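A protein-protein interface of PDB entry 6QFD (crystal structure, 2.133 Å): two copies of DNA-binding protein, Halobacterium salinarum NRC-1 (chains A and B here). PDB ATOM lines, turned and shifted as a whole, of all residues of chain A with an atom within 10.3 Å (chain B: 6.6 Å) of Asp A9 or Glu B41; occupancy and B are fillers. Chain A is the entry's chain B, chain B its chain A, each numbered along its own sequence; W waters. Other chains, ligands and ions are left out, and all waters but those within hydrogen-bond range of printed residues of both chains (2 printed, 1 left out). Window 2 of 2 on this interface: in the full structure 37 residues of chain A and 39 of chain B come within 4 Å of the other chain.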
ATOM      1  N   ASP A   2      18.611  -6.956  25.702  1.00  0.00           N
ATOM      2  CA  ASP A   2      17.657  -5.930  26.099  1.00  0.00           C
ATOM      3  C   ASP A   2      16.417  -6.019  25.218  1.00  0.00           C
ATOM      4  O   ASP A   2      16.519  -5.989  23.987  1.00  0.00           O
ATOM      5  CB  ASP A   2      18.279  -4.537  25.999  1.00  0.00           C
ATOM      6  CG  ASP A   2      17.413  -3.465  26.636  1.00  0.00           C
ATOM      7  OD1 ASP A   2      16.476  -3.823  27.381  1.00  0.00           O
ATOM      8  OD2 ASP A   2      17.666  -2.266  26.390  1.00  0.00           O
ATOM      9  N   ALA A   3      15.248  -6.133  25.854  1.00  0.00           N
ATOM     10  CA  ALA A   3      14.003  -6.232  25.102  1.00  0.00           C
ATOM     11  C   ALA A   3      13.674  -4.929  24.389  1.00  0.00           C
ATOM     12  O   ALA A   3      12.970  -4.940  23.371  1.00  0.00           O
ATOM     13  CB  ALA A   3      12.860  -6.631  26.033  1.00  0.00           C
ATOM     14  N   ARG A   4      14.161  -3.798  24.907  1.00  0.00           N
ATOM     15  CA  ARG A   4      13.953  -2.523  24.230  1.00  0.00           C
ATOM     16  C   ARG A   4      14.608  -2.522  22.853  1.00  0.00           C
ATOM     17  O   ARG A   4      14.010  -2.064  21.873  1.00  0.00           O
ATOM     18  CB  ARG A   4      14.511  -1.384  25.086  1.00  0.00           C
ATOM     19  CG  ARG A   4      13.456  -0.592  25.844  1.00  0.00           C
ATOM     20  CD  ARG A   4      14.094   0.408  26.796  1.00  0.00           C
ATOM     21  NE  ARG A   4      14.764  -0.251  27.916  1.00  0.00           N
ATOM     22  CZ  ARG A   4      14.246  -0.397  29.133  1.00  0.00           C
ATOM     23  NH1 ARG A   4      13.035   0.069  29.416  1.00  0.00           N
ATOM     24  NH2 ARG A   4      14.946  -1.015  30.076  1.00  0.00           N
ATOM     25  N   SER A   5      15.835  -3.040  22.761  1.00  0.00           N
ATOM     26  CA  SER A   5      16.560  -3.049  21.497  1.00  0.00           C
ATOM     27  C   SER A   5      15.860  -3.872  20.424  1.00  0.00           C
ATOM     28  O   SER A   5      16.163  -3.703  19.237  1.00  0.00           O
ATOM     29  CB  SER A   5      17.973  -3.597  21.710  1.00  0.00           C
ATOM     30  OG  SER A   5      18.582  -3.024  22.854  1.00  0.00           O
ATOM     31  N   ASP A   6      14.937  -4.755  20.809  1.00  0.00           N
ATOM     32  CA  ASP A   6      14.337  -5.702  19.882  1.00  0.00           C
ATOM     33  C   ASP A   6      12.839  -5.523  19.685  1.00  0.00           C
ATOM     34  O   ASP A   6      12.289  -6.104  18.742  1.00  0.00           O
ATOM     35  CB  ASP A   6      14.591  -7.143  20.358  1.00  0.00           C
ATOM     36  CG  ASP A   6      16.010  -7.607  20.093  1.00  0.00           C
ATOM     37  OD1 ASP A   6      16.957  -6.923  20.535  1.00  0.00           O
ATOM     38  OD2 ASP A   6      16.178  -8.662  19.446  1.00  0.00           O
ATOM     39  N   ALA A   7      12.167  -4.738  20.526  1.00  0.00           N
ATOM     40  CA  ALA A   7      10.711  -4.689  20.534  1.00  0.00           C
ATOM     41  C   ALA A   7      10.122  -3.351  20.103  1.00  0.00           C
ATOM     42  O   ALA A   7       8.898  -3.257  19.965  1.00  0.00           O
ATOM     43  CB  ALA A   7      10.187  -5.039  21.935  1.00  0.00           C
ATOM     44  N   ARG A   8      10.938  -2.328  19.875  1.00  0.00           N
ATOM     45  CA  ARG A   8      10.417  -1.037  19.464  1.00  0.00           C
ATOM     46  C   ARG A   8      10.233  -0.958  17.961  1.00  0.00           C
ATOM     47  O   ARG A   8       9.499  -0.085  17.506  1.00  0.00           O
ATOM     48  CB  ARG A   8      11.338   0.087  19.945  1.00  0.00           C
ATOM     49  CG  ARG A   8      11.436   0.158  21.445  1.00  0.00           C
ATOM     50  CD  ARG A   8      11.883   1.514  21.888  1.00  0.00           C
ATOM     51  NE  ARG A   8      11.719   1.582  23.316  1.00  0.00           N
ATOM     52  CZ  ARG A   8      12.039   2.614  24.070  1.00  0.00           C
ATOM     53  NH1 ARG A   8      12.555   3.719  23.581  1.00  0.00           N
ATOM     54  NH2 ARG A   8      11.843   2.511  25.350  1.00  0.00           N
ATOM     55  N   ASP A   9      10.845  -1.859  17.194  1.00  0.00           N
ATOM     56  CA  ASP A   9      10.700  -1.868  15.743  1.00  0.00           C
ATOM     57  C   ASP A   9       9.637  -2.856  15.272  1.00  0.00           C
ATOM     58  O   ASP A   9       9.323  -2.866  14.086  1.00  0.00           O
ATOM     59  CB  ASP A   9      12.054  -2.159  15.077  1.00  0.00           C
ATOM     60  CG  ASP A   9      12.896  -0.913  14.920  1.00  0.00           C
ATOM     61  OD1 ASP A   9      12.340   0.193  14.855  1.00  0.00           O
ATOM     62  OD2 ASP A   9      14.124  -1.043  14.868  1.00  0.00           O
ATOM     63  N   LEU A  10       8.996  -3.584  16.178  1.00  0.00           N
ATOM     64  CA  LEU A  10       7.972  -4.555  15.817  1.00  0.00           C
ATOM     65  C   LEU A  10       6.739  -3.857  15.270  1.00  0.00           C
ATOM     66  O   LEU A  10       6.437  -2.738  15.651  1.00  0.00           O
ATOM     67  CB  LEU A  10       7.547  -5.344  17.041  1.00  0.00           C
ATOM     68  CG  LEU A  10       8.638  -6.181  17.676  1.00  0.00           C
ATOM     69  CD1 LEU A  10       8.100  -6.823  18.939  1.00  0.00           C
ATOM     70  CD2 LEU A  10       9.215  -7.230  16.770  1.00  0.00           C
ATOM     71  N   THR A  11       5.975  -4.576  14.455  1.00  0.00           N
ATOM     72  CA  THR A  11       4.757  -4.043  13.866  1.00  0.00           C
ATOM     73  C   THR A  11       3.635  -4.132  14.894  1.00  0.00           C
ATOM     74  O   THR A  11       3.753  -4.823  15.898  1.00  0.00           O
ATOM     75  CB  THR A  11       4.378  -4.838  12.625  1.00  0.00           C
ATOM     76  OG1 THR A  11       3.768  -6.044  13.074  1.00  0.00           O
ATOM     77  CG2 THR A  11       5.575  -5.207  11.777  1.00  0.00           C
ATOM     78  N   ALA A  12       2.541  -3.418  14.645  1.00  0.00           N
ATOM     79  CA  ALA A  12       1.395  -3.482  15.547  1.00  0.00           C
ATOM     80  C   ALA A  12       0.894  -4.913  15.704  1.00  0.00           C
ATOM     81  O   ALA A  12       0.531  -5.337  16.809  1.00  0.00           O
ATOM     82  CB  ALA A  12       0.283  -2.580  15.017  1.00  0.00           C
ATOM     83  N   PHE A  13       0.868  -5.668  14.606  1.00  0.00           N
ATOM     84  CA  PHE A  13       0.450  -7.065  14.663  1.00  0.00           C
ATOM     85  C   PHE A  13       1.330  -7.858  15.622  1.00  0.00           C
ATOM     86  O   PHE A  13       0.830  -8.553  16.514  1.00  0.00           O
ATOM     87  CB  PHE A  13       0.497  -7.669  13.259  1.00  0.00           C
ATOM     88  CG  PHE A  13      -0.139  -9.026  13.156  1.00  0.00           C
ATOM     89  CD1 PHE A  13      -1.507  -9.178  13.304  1.00  0.00           C
ATOM     90  CD2 PHE A  13       0.632 -10.147  12.900  1.00  0.00           C
ATOM     91  CE1 PHE A  13      -2.092 -10.426  13.207  1.00  0.00           C
ATOM     92  CE2 PHE A  13       0.053 -11.395  12.802  1.00  0.00           C
ATOM     93  CZ  PHE A  13      -1.311 -11.535  12.955  1.00  0.00           C
ATOM     94  N   GLN A  14       2.650  -7.758  15.456  1.00  0.00           N
ATOM     95  CA  GLN A  14       3.564  -8.511  16.307  1.00  0.00           C
ATOM     96  C   GLN A  14       3.421  -8.103  17.767  1.00  0.00           C
ATOM     97  O   GLN A  14       3.422  -8.957  18.661  1.00  0.00           O
ATOM     98  CB  GLN A  14       5.003  -8.311  15.832  1.00  0.00           C
ATOM     99  CG  GLN A  14       5.290  -8.945  14.482  1.00  0.00           C
ATOM    100  CD  GLN A  14       6.668  -8.605  13.951  1.00  0.00           C
ATOM    101  OE1 GLN A  14       7.255  -7.585  14.314  1.00  0.00           O
ATOM    102  NE2 GLN A  14       7.192  -9.461  13.082  1.00  0.00           N
ATOM    103  N   LYS A  15       3.293  -6.802  18.030  1.00  0.00           N
ATOM    104  CA  LYS A  15       3.161  -6.344  19.409  1.00  0.00           C
ATOM    105  C   LYS A  15       1.858  -6.832  20.028  1.00  0.00           C
ATOM    106  O   LYS A  15       1.815  -7.156  21.220  1.00  0.00           O
ATOM    107  CB  LYS A  15       3.258  -4.819  19.463  1.00  0.00           C
ATOM    108  CG  LYS A  15       4.677  -4.301  19.249  1.00  0.00           C
ATOM    109  CD  LYS A  15       4.726  -2.833  18.843  1.00  0.00           C
ATOM    110  CE  LYS A  15       4.103  -1.916  19.883  1.00  0.00           C
ATOM    111  NZ  LYS A  15       3.162  -0.949  19.246  1.00  0.00           N
ATOM    112  N   LEU A  18       2.399 -10.386  21.223  1.00  0.00           N
ATOM    113  CA  LEU A  18       3.079 -10.418  22.513  1.00  0.00           C
ATOM    114  C   LEU A  18       2.121 -10.072  23.642  1.00  0.00           C
ATOM    115  O   LEU A  18       2.143 -10.705  24.704  1.00  0.00           O
ATOM    116  CB  LEU A  18       4.267  -9.457  22.510  1.00  0.00           C
ATOM    117  CG  LEU A  18       5.388  -9.738  21.504  1.00  0.00           C
ATOM    118  CD1 LEU A  18       6.459  -8.664  21.620  1.00  0.00           C
ATOM    119  CD2 LEU A  18       5.993 -11.115  21.704  1.00  0.00           C
ATOM    120  N   ASN A  51       4.671 -14.592  11.484  1.00  0.00           N
ATOM    121  CA  ASN A  51       4.967 -13.558  12.470  1.00  0.00           C
ATOM    122  C   ASN A  51       5.327 -14.167  13.820  1.00  0.00           C
ATOM    123  O   ASN A  51       6.179 -13.632  14.536  1.00  0.00           O
ATOM    124  CB  ASN A  51       3.781 -12.603  12.607  1.00  0.00           C
ATOM    125  CG  ASN A  51       3.854 -11.444  11.630  1.00  0.00           C
ATOM    126  OD1 ASN A  51       4.609 -10.492  11.833  1.00  0.00           O
ATOM    127  ND2 ASN A  51       3.073 -11.521  10.559  1.00  0.00           N
ATOM    128  N   ASP A  54       8.854 -15.136  13.365  1.00  0.00           N
ATOM    129  CA  ASP A  54       9.754 -13.994  13.496  1.00  0.00           C
ATOM    130  C   ASP A  54      10.001 -13.666  14.963  1.00  0.00           C
ATOM    131  O   ASP A  54      11.149 -13.499  15.388  1.00  0.00           O
ATOM    132  CB  ASP A  54       9.177 -12.779  12.767  1.00  0.00           C
ATOM    133  CG  ASP A  54       9.353 -12.860  11.261  1.00  0.00           C
ATOM    134  OD1 ASP A  54       9.786 -13.921  10.764  1.00  0.00           O
ATOM    135  OD2 ASP A  54       9.057 -11.858  10.575  1.00  0.00           O
ATOM    136  N   LEU A  55       8.930 -13.571  15.755  1.00  0.00           N
ATOM    137  CA  LEU A  55       9.084 -13.310  17.180  1.00  0.00           C
ATOM    138  C   LEU A  55       9.943 -14.373  17.851  1.00  0.00           C
ATOM    139  O   LEU A  55      10.655 -14.077  18.818  1.00  0.00           O
ATOM    140  CB  LEU A  55       7.712 -13.240  17.850  1.00  0.00           C
ATOM    141  CG  LEU A  55       6.874 -12.004  17.517  1.00  0.00           C
ATOM    142  CD1 LEU A  55       5.461 -12.143  18.065  1.00  0.00           C
ATOM    143  CD2 LEU A  55       7.543 -10.753  18.056  1.00  0.00           C
ATOM    144  N   LYS A  58      13.529 -13.576  16.982  1.00  0.00           N
ATOM    145  CA  LYS A  58      13.973 -12.369  17.665  1.00  0.00           C
ATOM    146  C   LYS A  58      14.260 -12.616  19.135  1.00  0.00           C
ATOM    147  O   LYS A  58      14.811 -11.732  19.784  1.00  0.00           O
ATOM    148  CB  LYS A  58      12.923 -11.259  17.519  1.00  0.00           C
ATOM    149  CG  LYS A  58      13.074 -10.464  16.242  1.00  0.00           C
ATOM    150  CD  LYS A  58      11.847  -9.689  15.908  1.00  0.00           C
ATOM    151  CE  LYS A  58      12.100  -8.808  14.716  1.00  0.00           C
ATOM    152  NZ  LYS A  58      13.292  -7.954  14.930  1.00  0.00           N
ATOM    153  N   LEU A  60      11.880 -13.337  21.460  1.00  0.00           N
ATOM    154  CA  LEU A  60      10.768 -12.865  22.287  1.00  0.00           C
ATOM    155  C   LEU A  60       9.703 -13.927  22.539  1.00  0.00           C
ATOM    156  O   LEU A  60       8.868 -13.745  23.432  1.00  0.00           O
ATOM    157  CB  LEU A  60      10.118 -11.643  21.618  1.00  0.00           C
ATOM    158  CG  LEU A  60      11.106 -10.587  21.107  1.00  0.00           C
ATOM    159  CD1 LEU A  60      10.378  -9.420  20.462  1.00  0.00           C
ATOM    160  CD2 LEU A  60      12.003 -10.093  22.236  1.00  0.00           C
ATOM    161  N   ALA A  82       9.787  -7.149  26.934  1.00  0.00           N
ATOM    162  CA  ALA A  82       9.286  -6.330  25.836  1.00  0.00           C
ATOM    163  C   ALA A  82       7.882  -5.818  26.130  1.00  0.00           C
ATOM    164  O   ALA A  82       7.572  -4.649  25.876  1.00  0.00           O
ATOM    165  CB  ALA A  82       9.298  -7.131  24.533  1.00  0.00           C
ATOM    166  N   ASP A  86       7.029  -1.783  26.695  1.00  0.00           N
ATOM    167  CA  ASP A  86       6.032  -1.063  25.909  1.00  0.00           C
ATOM    168  C   ASP A  86       4.975  -0.434  26.808  1.00  0.00           C
ATOM    169  O   ASP A  86       4.491   0.671  26.531  1.00  0.00           O
ATOM    170  CB  ASP A  86       5.378  -2.002  24.898  1.00  0.00           C
ATOM    171  CG  ASP A  86       4.349  -1.299  24.032  1.00  0.00           C
ATOM    172  OD1 ASP A  86       4.743  -0.436  23.216  1.00  0.00           O
ATOM    173  OD2 ASP A  86       3.144  -1.606  24.171  1.00  0.00           O
ATOM    174  N   ALA B  12       1.873   0.783  14.056  1.00  0.00           N
ATOM    175  CA  ALA B  12       2.655   1.092  15.247  1.00  0.00           C
ATOM    176  C   ALA B  12       3.170   2.524  15.205  1.00  0.00           C
ATOM    177  O   ALA B  12       3.105   3.246  16.208  1.00  0.00           O
ATOM    178  CB  ALA B  12       3.820   0.112  15.381  1.00  0.00           C
ATOM    179  N   LYS B  32       8.660  14.606  15.846  1.00  0.00           N
ATOM    180  CA  LYS B  32       9.748  13.877  15.207  1.00  0.00           C
ATOM    181  C   LYS B  32      10.859  13.566  16.201  1.00  0.00           C
ATOM    182  O   LYS B  32      11.311  12.420  16.306  1.00  0.00           O
ATOM    183  CB  LYS B  32      10.286  14.694  14.033  1.00  0.00           C
ATOM    184  CG  LYS B  32      11.203  13.927  13.107  1.00  0.00           C
ATOM    185  CD  LYS B  32      11.694  14.808  11.972  1.00  0.00           C
ATOM    186  CE  LYS B  32      13.107  14.433  11.559  1.00  0.00           C
ATOM    187  NZ  LYS B  32      14.146  15.195  12.302  1.00  0.00           N
ATOM    188  N   LEU B  35       9.938  10.875  18.734  1.00  0.00           N
ATOM    189  CA  LEU B  35       9.965   9.529  18.181  1.00  0.00           C
ATOM    190  C   LEU B  35      11.393   9.089  17.872  1.00  0.00           C
ATOM    191  O   LEU B  35      11.715   7.906  18.000  1.00  0.00           O
ATOM    192  CB  LEU B  35       9.098   9.442  16.929  1.00  0.00           C
ATOM    193  CG  LEU B  35       7.624   9.809  17.109  1.00  0.00           C
ATOM    194  CD1 LEU B  35       6.971  10.088  15.762  1.00  0.00           C
ATOM    195  CD2 LEU B  35       6.875   8.707  17.842  1.00  0.00           C
ATOM    196  N   GLU B  36      12.270  10.025  17.496  1.00  0.00           N
ATOM    197  CA  GLU B  36      13.673   9.672  17.301  1.00  0.00           C
ATOM    198  C   GLU B  36      14.319   9.235  18.609  1.00  0.00           C
ATOM    199  O   GLU B  36      15.213   8.380  18.606  1.00  0.00           O
ATOM    200  CB  GLU B  36      14.431  10.855  16.696  1.00  0.00           C
ATOM    201  CG  GLU B  36      14.076  11.126  15.240  1.00  0.00           C
ATOM    202  CD  GLU B  36      14.725  12.387  14.692  1.00  0.00           C
ATOM    203  OE1 GLU B  36      14.464  13.481  15.238  1.00  0.00           O
ATOM    204  OE2 GLU B  36      15.490  12.283  13.710  1.00  0.00           O
ATOM    205  N   GLU B  37      13.884   9.804  19.735  1.00  0.00           N
ATOM    206  CA  GLU B  37      14.381   9.350  21.028  1.00  0.00           C
ATOM    207  C   GLU B  37      13.803   7.990  21.392  1.00  0.00           C
ATOM    208  O   GLU B  37      14.461   7.199  22.079  1.00  0.00           O
ATOM    209  CB  GLU B  37      14.046  10.374  22.111  1.00  0.00           C
ATOM    210  CG  GLU B  37      14.952  10.298  23.330  1.00  0.00           C
ATOM    211  CD  GLU B  37      16.276  11.012  23.128  1.00  0.00           C
ATOM    212  OE1 GLU B  37      16.518  11.531  22.017  1.00  0.00           O
ATOM    213  OE2 GLU B  37      17.075  11.056  24.087  1.00  0.00           O
ATOM    214  N   TYR B  38      12.581   7.702  20.942  1.00  0.00           N
ATOM    215  CA  TYR B  38      11.970   6.405  21.204  1.00  0.00           C
ATOM    216  C   TYR B  38      12.615   5.318  20.353  1.00  0.00           C
ATOM    217  O   TYR B  38      13.098   4.306  20.873  1.00  0.00           O
ATOM    218  CB  TYR B  38      10.466   6.476  20.934  1.00  0.00           C
ATOM    219  CG  TYR B  38       9.782   5.130  20.962  1.00  0.00           C
ATOM    220  CD1 TYR B  38       9.363   4.571  22.158  1.00  0.00           C
ATOM    221  CD2 TYR B  38       9.562   4.416  19.791  1.00  0.00           C
ATOM    222  CE1 TYR B  38       8.739   3.339  22.191  1.00  0.00           C
ATOM    223  CE2 TYR B  38       8.939   3.184  19.813  1.00  0.00           C
ATOM    224  CZ  TYR B  38       8.532   2.648  21.014  1.00  0.00           C
ATOM    225  OH  TYR B  38       7.909   1.421  21.040  1.00  0.00           O
ATOM    226  N   TYR B  39      12.630   5.512  19.032  1.00  0.00           N
ATOM    227  CA  TYR B  39      13.187   4.508  18.136  1.00  0.00           C
ATOM    228  C   TYR B  39      14.703   4.404  18.240  1.00  0.00           C
ATOM    229  O   TYR B  39      15.266   3.370  17.865  1.00  0.00           O
ATOM    230  CB  TYR B  39      12.806   4.826  16.687  1.00  0.00           C
ATOM    231  CG  TYR B  39      11.349   4.598  16.362  1.00  0.00           C
ATOM    232  CD1 TYR B  39      10.779   3.338  16.483  1.00  0.00           C
ATOM    233  CD2 TYR B  39      10.545   5.640  15.926  1.00  0.00           C
ATOM    234  CE1 TYR B  39       9.446   3.126  16.185  1.00  0.00           C
ATOM    235  CE2 TYR B  39       9.211   5.436  15.624  1.00  0.00           C
ATOM    236  CZ  TYR B  39       8.668   4.180  15.756  1.00  0.00           C
ATOM    237  OH  TYR B  39       7.342   3.973  15.457  1.00  0.00           O
ATOM    238  N   GLY B  40      15.377   5.439  18.733  1.00  0.00           N
ATOM    239  CA  GLY B  40      16.827   5.464  18.666  1.00  0.00           C
ATOM    240  C   GLY B  40      17.343   5.491  17.247  1.00  0.00           C
ATOM    241  O   GLY B  40      18.457   5.024  16.982  1.00  0.00           O
ATOM    242  N   GLU B  41      16.542   6.009  16.320  1.00  0.00           N
ATOM    243  CA  GLU B  41      16.889   6.078  14.911  1.00  0.00           C
ATOM    244  C   GLU B  41      16.387   7.407  14.368  1.00  0.00           C
ATOM    245  O   GLU B  41      15.468   8.016  14.922  1.00  0.00           O
ATOM    246  CB  GLU B  41      16.270   4.924  14.101  1.00  0.00           C
ATOM    247  CG  GLU B  41      16.437   3.533  14.709  1.00  0.00           C
ATOM    248  CD  GLU B  41      15.258   2.610  14.413  1.00  0.00           C
ATOM    249  OE1 GLU B  41      14.361   3.000  13.633  1.00  0.00           O
ATOM    250  OE2 GLU B  41      15.228   1.490  14.967  1.00  0.00           O
ATOM    251  N   GLU B  42      16.993   7.856  13.275  1.00  0.00           N
ATOM    252  CA  GLU B  42      16.495   9.042  12.595  1.00  0.00           C
ATOM    253  C   GLU B  42      15.134   8.739  11.976  1.00  0.00           C
ATOM    254  O   GLU B  42      14.939   7.685  11.360  1.00  0.00           O
ATOM    255  CB  GLU B  42      17.478   9.507  11.521  1.00  0.00           C
ATOM    256  CG  GLU B  42      18.930   9.616  11.984  1.00  0.00           C
ATOM    257  CD  GLU B  42      19.221  10.909  12.728  1.00  0.00           C
ATOM    258  OE1 GLU B  42      20.383  11.367  12.695  1.00  0.00           O
ATOM    259  OE2 GLU B  42      18.288  11.462  13.349  1.00  0.00           O
ATOM    260  N   VAL B  43      14.189   9.657  12.152  1.00  0.00           N
ATOM    261  CA  VAL B  43      12.832   9.508  11.635  1.00  0.00           C
ATOM    262  C   VAL B  43      12.670  10.467  10.465  1.00  0.00           C
ATOM    263  O   VAL B  43      12.793  11.684  10.632  1.00  0.00           O
ATOM    264  CB  VAL B  43      11.778   9.780  12.719  1.00  0.00           C
ATOM    265  CG1 VAL B  43      10.392   9.896  12.096  1.00  0.00           C
ATOM    266  CG2 VAL B  43      11.803   8.686  13.774  1.00  0.00           C
ATOM    267  N   ARG B  47       8.154  10.733   6.143  1.00  0.00           N
ATOM    268  CA  ARG B  47       7.284   9.696   6.681  1.00  0.00           C
ATOM    269  C   ARG B  47       6.300  10.258   7.696  1.00  0.00           C
ATOM    270  O   ARG B  47       5.153   9.803   7.770  1.00  0.00           O
ATOM    271  CB  ARG B  47       8.117   8.593   7.338  1.00  0.00           C
ATOM    272  CG  ARG B  47       7.287   7.472   7.946  1.00  0.00           C
ATOM    273  CD  ARG B  47       8.127   6.539   8.800  1.00  0.00           C
ATOM    274  NE  ARG B  47       7.416   5.294   9.074  1.00  0.00           N
ATOM    275  CZ  ARG B  47       7.807   4.381   9.956  1.00  0.00           C
ATOM    276  NH1 ARG B  47       8.911   4.562  10.668  1.00  0.00           N
ATOM    277  NH2 ARG B  47       7.085   3.282  10.127  1.00  0.00           N
HETATM  278  O   HOH W   1       2.965  -1.361  12.188  1.00  0.00           O
HETATM  279  O   HOH W   2       6.396   0.782  18.757  1.00  0.00           O
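Water W2 bridges the side-chain hydroxyl (OH) of Tyr B38 and the backbone carbonyl oxygen (O) of Arg A8.
Water W1 bridges the backbone NH (N) of Ala B12 and the backbone NH (N) of Ala A12.
Arg A8 touches Tyr B39.
Tyr B39 touches Asp A9 (CD1 to OD1, 3.9 Å).
Leu A10 touches Ala B12 (O to CB, 3.9 Å).
N of Ala A12 touches CB of Ala B12, 3.8 Å away.
Of the 12 printed residues of chain B, 4 touch a printed residue of chain A.
Hydrophobic or aromatic side chains of chain B that line the printed part of chain A: Ala B12, Tyr B38 and Tyr B39.
Hydrophobic or aromatic side chains of chain A that line the printed part of chain B: Ala A12.
Among the printed residues, no Asp or Glu carboxylate lies within 4 Å of a Lys or Arg side-chain nitrogen of the other chain.
Ala A12 touches its own counterpart, Ala B12.
Position printed for both chains: 12.
Of the 6 pairs that touch across the chains among the printed residues, 1 has its exchanged pair printed and touching as well.
The guanidinium group (NH1) of Arg A8 is in hydrogen-bond range of the backbone carbonyl oxygen (O) of Tyr B38, at 2.8 Å.
OE2 of Glu B41 sits close to OD2 of Asp A9 (2.8 Å).
Asp A9 touches just these residues of chain B: Tyr B39 and Glu B41.
Glu B41 touches one residue of chain A.
Gly B40 touches none of the printed residues of chain A.
No residue of chain A comes within 4 Å of Val B43.
Printed residues of chain A within 4 Å of Tyr B38: Arg A8.
Printed residues of chain B within 4 Å of Leu A10: Ala B12.
Of the printed residues of chain B, Arg A8 touches Tyr B38 (2.8 Å) and Tyr B39 (3.5 Å).
Of the printed residues of chain A, Ala B12 touches Leu A10 and Ala A12.
The nearest residue of chain B that does not touch Asp A9 is Tyr B38 (5.8 Å).
The nearest residue of chain A that does not touch Glu B41 is Arg A8 (6.3 Å).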
